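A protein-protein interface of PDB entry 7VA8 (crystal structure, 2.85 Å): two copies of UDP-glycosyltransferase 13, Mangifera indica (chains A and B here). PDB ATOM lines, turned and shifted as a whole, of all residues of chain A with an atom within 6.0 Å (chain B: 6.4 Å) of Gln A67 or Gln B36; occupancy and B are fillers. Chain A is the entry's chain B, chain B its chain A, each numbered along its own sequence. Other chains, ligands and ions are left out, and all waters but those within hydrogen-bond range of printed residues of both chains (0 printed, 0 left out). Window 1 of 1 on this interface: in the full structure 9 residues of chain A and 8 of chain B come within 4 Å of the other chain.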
ATOM      1  N   VAL A  35     -17.477 -35.675 -27.157  1.00  0.00           N
ATOM      2  CA  VAL A  35     -16.969 -34.379 -26.723  1.00  0.00           C
ATOM      3  C   VAL A  35     -17.266 -33.320 -27.779  1.00  0.00           C
ATOM      4  O   VAL A  35     -17.692 -32.208 -27.461  1.00  0.00           O
ATOM      5  CB  VAL A  35     -15.454 -34.431 -26.443  1.00  0.00           C
ATOM      6  CG1 VAL A  35     -14.871 -33.022 -26.353  1.00  0.00           C
ATOM      7  CG2 VAL A  35     -15.184 -35.201 -25.162  1.00  0.00           C
ATOM      8  N   ARG A  40     -20.142 -34.096 -21.963  1.00  0.00           N
ATOM      9  CA  ARG A  40     -19.026 -34.351 -21.061  1.00  0.00           C
ATOM     10  C   ARG A  40     -18.742 -35.838 -21.102  1.00  0.00           C
ATOM     11  O   ARG A  40     -19.661 -36.645 -21.122  1.00  0.00           O
ATOM     12  CB  ARG A  40     -19.336 -33.896 -19.636  1.00  0.00           C
ATOM     13  CG  ARG A  40     -18.168 -34.055 -18.675  1.00  0.00           C
ATOM     14  CD  ARG A  40     -18.463 -33.350 -17.367  1.00  0.00           C
ATOM     15  NE  ARG A  40     -19.193 -32.111 -17.608  1.00  0.00           N
ATOM     16  CZ  ARG A  40     -19.115 -31.027 -16.846  1.00  0.00           C
ATOM     17  NH1 ARG A  40     -19.823 -29.952 -17.161  1.00  0.00           N
ATOM     18  NH2 ARG A  40     -18.329 -31.012 -15.779  1.00  0.00           N
ATOM     19  N   VAL A  41     -17.468 -36.201 -21.134  1.00  0.00           N
ATOM     20  CA  VAL A  41     -17.087 -37.599 -21.273  1.00  0.00           C
ATOM     21  C   VAL A  41     -16.141 -38.049 -20.172  1.00  0.00           C
ATOM     22  O   VAL A  41     -15.116 -37.420 -19.923  1.00  0.00           O
ATOM     23  CB  VAL A  41     -16.428 -37.856 -22.643  1.00  0.00           C
ATOM     24  CG1 VAL A  41     -15.623 -39.149 -22.622  1.00  0.00           C
ATOM     25  CG2 VAL A  41     -17.483 -37.884 -23.737  1.00  0.00           C
ATOM     26  N   LEU A  62      -6.185 -38.254 -23.555  1.00  0.00           N
ATOM     27  CA  LEU A  62      -6.272 -37.434 -22.353  1.00  0.00           C
ATOM     28  C   LEU A  62      -5.443 -36.163 -22.485  1.00  0.00           C
ATOM     29  O   LEU A  62      -5.788 -35.126 -21.918  1.00  0.00           O
ATOM     30  CB  LEU A  62      -5.823 -38.230 -21.127  1.00  0.00           C
ATOM     31  CG  LEU A  62      -6.729 -39.388 -20.705  1.00  0.00           C
ATOM     32  CD1 LEU A  62      -6.133 -40.127 -19.519  1.00  0.00           C
ATOM     33  CD2 LEU A  62      -8.131 -38.890 -20.384  1.00  0.00           C
ATOM     34  N   ASP A  64      -4.780 -34.606 -25.501  1.00  0.00           N
ATOM     35  CA  ASP A  64      -5.455 -33.763 -26.479  1.00  0.00           C
ATOM     36  C   ASP A  64      -6.791 -33.247 -25.956  1.00  0.00           C
ATOM     37  O   ASP A  64      -7.257 -32.186 -26.366  1.00  0.00           O
ATOM     38  CB  ASP A  64      -5.660 -34.524 -27.792  1.00  0.00           C
ATOM     39  CG  ASP A  64      -4.449 -34.444 -28.703  1.00  0.00           C
ATOM     40  OD1 ASP A  64      -3.313 -34.555 -28.192  1.00  0.00           O
ATOM     41  OD2 ASP A  64      -4.635 -34.264 -29.926  1.00  0.00           O
ATOM     42  N   PHE A  65      -7.403 -34.000 -25.048  1.00  0.00           N
ATOM     43  CA  PHE A  65      -8.694 -33.617 -24.490  1.00  0.00           C
ATOM     44  C   PHE A  65      -8.644 -33.483 -22.974  1.00  0.00           C
ATOM     45  O   PHE A  65      -8.979 -34.423 -22.255  1.00  0.00           O
ATOM     46  CB  PHE A  65      -9.766 -34.633 -24.882  1.00  0.00           C
ATOM     47  CG  PHE A  65     -10.060 -34.667 -26.352  1.00  0.00           C
ATOM     48  CD1 PHE A  65      -9.270 -35.408 -27.213  1.00  0.00           C
ATOM     49  CD2 PHE A  65     -11.129 -33.959 -26.872  1.00  0.00           C
ATOM     50  CE1 PHE A  65      -9.538 -35.442 -28.567  1.00  0.00           C
ATOM     51  CE2 PHE A  65     -11.405 -33.985 -28.222  1.00  0.00           C
ATOM     52  CZ  PHE A  65     -10.608 -34.729 -29.073  1.00  0.00           C
ATOM     53  N   PRO A  66      -8.220 -32.310 -22.481  1.00  0.00           N
ATOM     54  CA  PRO A  66      -8.208 -32.053 -21.038  1.00  0.00           C
ATOM     55  C   PRO A  66      -9.606 -32.075 -20.426  1.00  0.00           C
ATOM     56  O   PRO A  66      -9.733 -32.197 -19.206  1.00  0.00           O
ATOM     57  CB  PRO A  66      -7.589 -30.659 -20.934  1.00  0.00           C
ATOM     58  CG  PRO A  66      -6.774 -30.514 -22.183  1.00  0.00           C
ATOM     59  CD  PRO A  66      -7.545 -31.242 -23.239  1.00  0.00           C
ATOM     60  N   GLN A  67     -10.640 -31.964 -21.254  1.00  0.00           N
ATOM     61  CA  GLN A  67     -12.013 -31.948 -20.753  1.00  0.00           C
ATOM     62  C   GLN A  67     -12.585 -33.355 -20.586  1.00  0.00           C
ATOM     63  O   GLN A  67     -13.779 -33.518 -20.358  1.00  0.00           O
ATOM     64  CB  GLN A  67     -12.919 -31.129 -21.680  1.00  0.00           C
ATOM     65  CG  GLN A  67     -12.995 -31.627 -23.119  1.00  0.00           C
ATOM     66  CD  GLN A  67     -11.829 -31.157 -23.964  1.00  0.00           C
ATOM     67  OE1 GLN A  67     -10.702 -31.036 -23.485  1.00  0.00           O
ATOM     68  NE2 GLN A  67     -12.098 -30.883 -25.233  1.00  0.00           N
ATOM     69  N   ILE A  68     -11.731 -34.366 -20.702  1.00  0.00           N
ATOM     70  CA  ILE A  68     -12.140 -35.745 -20.469  1.00  0.00           C
ATOM     71  C   ILE A  68     -11.535 -36.247 -19.165  1.00  0.00           C
ATOM     72  O   ILE A  68     -10.336 -36.110 -18.939  1.00  0.00           O
ATOM     73  CB  ILE A  68     -11.719 -36.670 -21.631  1.00  0.00           C
ATOM     74  CG1 ILE A  68     -12.563 -36.385 -22.875  1.00  0.00           C
ATOM     75  CG2 ILE A  68     -11.844 -38.135 -21.236  1.00  0.00           C
ATOM     76  CD1 ILE A  68     -12.360 -37.392 -23.987  1.00  0.00           C
ATOM     77  N   THR A  69     -12.371 -36.815 -18.301  1.00  0.00           N
ATOM     78  CA  THR A  69     -11.913 -37.331 -17.012  1.00  0.00           C
ATOM     79  C   THR A  69     -11.663 -38.834 -17.064  1.00  0.00           C
ATOM     80  O   THR A  69     -12.421 -39.577 -17.684  1.00  0.00           O
ATOM     81  CB  THR A  69     -12.935 -37.031 -15.893  1.00  0.00           C
ATOM     82  OG1 THR A  69     -13.336 -35.656 -15.960  1.00  0.00           O
ATOM     83  CG2 THR A  69     -12.332 -37.307 -14.518  1.00  0.00           C
ATOM     84  N   ALA B  31     -10.867 -19.063 -26.598  1.00  0.00           N
ATOM     85  CA  ALA B  31     -11.946 -19.956 -27.009  1.00  0.00           C
ATOM     86  C   ALA B  31     -11.576 -21.402 -26.697  1.00  0.00           C
ATOM     87  O   ALA B  31     -12.395 -22.173 -26.194  1.00  0.00           O
ATOM     88  CB  ALA B  31     -12.240 -19.783 -28.488  1.00  0.00           C
ATOM     89  N   ALA B  32     -10.327 -21.754 -26.988  1.00  0.00           N
ATOM     90  CA  ALA B  32      -9.832 -23.102 -26.732  1.00  0.00           C
ATOM     91  C   ALA B  32      -9.869 -23.414 -25.242  1.00  0.00           C
ATOM     92  O   ALA B  32     -10.311 -24.487 -24.837  1.00  0.00           O
ATOM     93  CB  ALA B  32      -8.425 -23.263 -27.269  1.00  0.00           C
ATOM     94  N   THR B  33      -9.409 -22.467 -24.429  1.00  0.00           N
ATOM     95  CA  THR B  33      -9.416 -22.634 -22.976  1.00  0.00           C
ATOM     96  C   THR B  33     -10.833 -22.809 -22.438  1.00  0.00           C
ATOM     97  O   THR B  33     -11.095 -23.697 -21.619  1.00  0.00           O
ATOM     98  CB  THR B  33      -8.756 -21.434 -22.273  1.00  0.00           C
ATOM     99  OG1 THR B  33      -7.441 -21.235 -22.805  1.00  0.00           O
ATOM    100  CG2 THR B  33      -8.653 -21.688 -20.778  1.00  0.00           C
ATOM    101  N   LEU B  34     -11.745 -21.958 -22.902  1.00  0.00           N
ATOM    102  CA  LEU B  34     -13.143 -22.028 -22.489  1.00  0.00           C
ATOM    103  C   LEU B  34     -13.765 -23.376 -22.814  1.00  0.00           C
ATOM    104  O   LEU B  34     -14.403 -23.993 -21.967  1.00  0.00           O
ATOM    105  CB  LEU B  34     -13.959 -20.929 -23.160  1.00  0.00           C
ATOM    106  CG  LEU B  34     -13.861 -19.507 -22.622  1.00  0.00           C
ATOM    107  CD1 LEU B  34     -14.876 -18.636 -23.343  1.00  0.00           C
ATOM    108  CD2 LEU B  34     -14.097 -19.487 -21.124  1.00  0.00           C
ATOM    109  N   VAL B  35     -13.585 -23.820 -24.053  1.00  0.00           N
ATOM    110  CA  VAL B  35     -14.096 -25.120 -24.476  1.00  0.00           C
ATOM    111  C   VAL B  35     -13.495 -26.227 -23.619  1.00  0.00           C
ATOM    112  O   VAL B  35     -14.187 -27.163 -23.217  1.00  0.00           O
ATOM    113  CB  VAL B  35     -13.790 -25.394 -25.960  1.00  0.00           C
ATOM    114  CG1 VAL B  35     -14.164 -26.826 -26.328  1.00  0.00           C
ATOM    115  CG2 VAL B  35     -14.540 -24.414 -26.838  1.00  0.00           C
ATOM    116  N   GLN B  36     -12.208 -26.103 -23.317  1.00  0.00           N
ATOM    117  CA  GLN B  36     -11.517 -27.107 -22.516  1.00  0.00           C
ATOM    118  C   GLN B  36     -11.840 -26.968 -21.036  1.00  0.00           C
ATOM    119  O   GLN B  36     -11.327 -27.714 -20.206  1.00  0.00           O
ATOM    120  CB  GLN B  36     -10.008 -27.018 -22.745  1.00  0.00           C
ATOM    121  CG  GLN B  36      -9.555 -27.684 -24.027  1.00  0.00           C
ATOM    122  CD  GLN B  36      -8.110 -27.394 -24.347  1.00  0.00           C
ATOM    123  OE1 GLN B  36      -7.455 -26.620 -23.653  1.00  0.00           O
ATOM    124  NE2 GLN B  36      -7.603 -28.013 -25.406  1.00  0.00           N
ATOM    125  N   HIS B  37     -12.695 -26.004 -20.712  1.00  0.00           N
ATOM    126  CA  HIS B  37     -13.227 -25.879 -19.358  1.00  0.00           C
ATOM    127  C   HIS B  37     -14.753 -25.969 -19.356  1.00  0.00           C
ATOM    128  O   HIS B  37     -15.426 -25.256 -18.615  1.00  0.00           O
ATOM    129  CB  HIS B  37     -12.766 -24.571 -18.711  1.00  0.00           C
ATOM    130  CG  HIS B  37     -11.403 -24.653 -18.094  1.00  0.00           C
ATOM    131  ND1 HIS B  37     -10.244 -24.567 -18.830  1.00  0.00           N
ATOM    132  CD2 HIS B  37     -11.019 -24.819 -16.804  1.00  0.00           C
ATOM    133  CE1 HIS B  37      -9.201 -24.671 -18.021  1.00  0.00           C
ATOM    134  NE2 HIS B  37      -9.647 -24.826 -16.788  1.00  0.00           N
ATOM    135  N   HIS B  38     -15.278 -26.852 -20.203  1.00  0.00           N
ATOM    136  CA  HIS B  38     -16.703 -27.184 -20.241  1.00  0.00           C
ATOM    137  C   HIS B  38     -17.613 -25.974 -20.454  1.00  0.00           C
ATOM    138  O   HIS B  38     -18.560 -25.758 -19.701  1.00  0.00           O
ATOM    139  CB  HIS B  38     -17.103 -27.917 -18.956  1.00  0.00           C
ATOM    140  CG  HIS B  38     -16.216 -29.063 -18.613  1.00  0.00           C
ATOM    141  ND1 HIS B  38     -15.393 -29.077 -17.509  1.00  0.00           N
ATOM    142  CD2 HIS B  38     -16.006 -30.261 -19.240  1.00  0.00           C
ATOM    143  CE1 HIS B  38     -14.725 -30.216 -17.460  1.00  0.00           C
ATOM    144  NE2 HIS B  38     -15.085 -30.944 -18.505  1.00  0.00           N
ATOM    145  N   CYS B  39     -17.313 -25.189 -21.484  1.00  0.00           N
ATOM    146  CA  CYS B  39     -18.163 -24.071 -21.888  1.00  0.00           C
ATOM    147  C   CYS B  39     -18.460 -24.146 -23.379  1.00  0.00           C
ATOM    148  O   CYS B  39     -17.650 -24.650 -24.153  1.00  0.00           O
ATOM    149  CB  CYS B  39     -17.507 -22.729 -21.561  1.00  0.00           C
ATOM    150  SG  CYS B  39     -17.638 -22.212 -19.836  1.00  0.00           S
ATOM    151  N   PHE B  65     -11.494 -28.169 -33.234  1.00  0.00           N
ATOM    152  CA  PHE B  65     -12.639 -28.051 -32.333  1.00  0.00           C
ATOM    153  C   PHE B  65     -13.952 -27.924 -33.096  1.00  0.00           C
ATOM    154  O   PHE B  65     -14.439 -26.821 -33.318  1.00  0.00           O
ATOM    155  CB  PHE B  65     -12.472 -26.850 -31.402  1.00  0.00           C
ATOM    156  CG  PHE B  65     -11.261 -26.924 -30.527  1.00  0.00           C
ATOM    157  CD1 PHE B  65     -10.056 -26.394 -30.950  1.00  0.00           C
ATOM    158  CD2 PHE B  65     -11.328 -27.514 -29.278  1.00  0.00           C
ATOM    159  CE1 PHE B  65      -8.936 -26.455 -30.148  1.00  0.00           C
ATOM    160  CE2 PHE B  65     -10.215 -27.581 -28.467  1.00  0.00           C
ATOM    161  CZ  PHE B  65      -9.014 -27.050 -28.902  1.00  0.00           C
ATOM    162  N   GLN B  67     -16.829 -28.526 -32.091  1.00  0.00           N
ATOM    163  CA  GLN B  67     -17.937 -28.121 -31.225  1.00  0.00           C
ATOM    164  C   GLN B  67     -18.024 -26.609 -31.062  1.00  0.00           C
ATOM    165  O   GLN B  67     -18.874 -26.110 -30.333  1.00  0.00           O
ATOM    166  CB  GLN B  67     -17.818 -28.783 -29.843  1.00  0.00           C
ATOM    167  CG  GLN B  67     -16.607 -28.366 -29.027  1.00  0.00           C
ATOM    168  CD  GLN B  67     -15.358 -29.134 -29.403  1.00  0.00           C
ATOM    169  OE1 GLN B  67     -15.108 -29.395 -30.579  1.00  0.00           O
ATOM    170  NE2 GLN B  67     -14.566 -29.502 -28.403  1.00  0.00           N
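The backbone carbonyl oxygen (O) of Gln A67 is in hydrogen-bond range of a ring nitrogen (NE2) of His B38 (3.4 Å).
Among the printed residues, merely in contact across the chains: Gln A67 with Gln B36, Arg A40 with His B38 and Pro A66 with Gln B36.
Printed residues of chain B within 4 Å of Arg A40: His B38 (3.8 Å).
Of chain B, only Gln B36 (3.6 Å) and His B38 (3.4 Å) come within 4 Å of Gln A67.
Gln B36 touches just these residues of chain A: Pro A66 (3.9 Å) and Gln A67 (3.6 Å).
Printed residues of chain A within 4 Å of His B38: Arg A40 (3.8 Å) and Gln A67 (3.4 Å).
Gln B67 touches none of the printed residues of chain A.
The nearest residue of chain B that does not touch Gln A67 is Gln B67 (4.2 Å).
The nearest residue of chain A that does not touch Gln B36 is Asp A64 (4.3 Å).
Printed residues of chain A that touch a printed residue of chain B: Arg A40, Pro A66 and Gln A67.
Hydrophobic or aromatic side chains of chain A within 4 Å of the printed part of chain B: Pro A66.
Of the 11 printed residues of chain B, 2 touch a printed residue of chain A.
Among the printed residues, no Asp or Glu carboxylate lies within 4 Å of a Lys or Arg side-chain nitrogen of the other chain.
Positions printed for both chains: 35, 65 and 67.
Of the 4 pairs that touch across the chains among the printed residues, none has its exchanged pair printed and touching as well.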
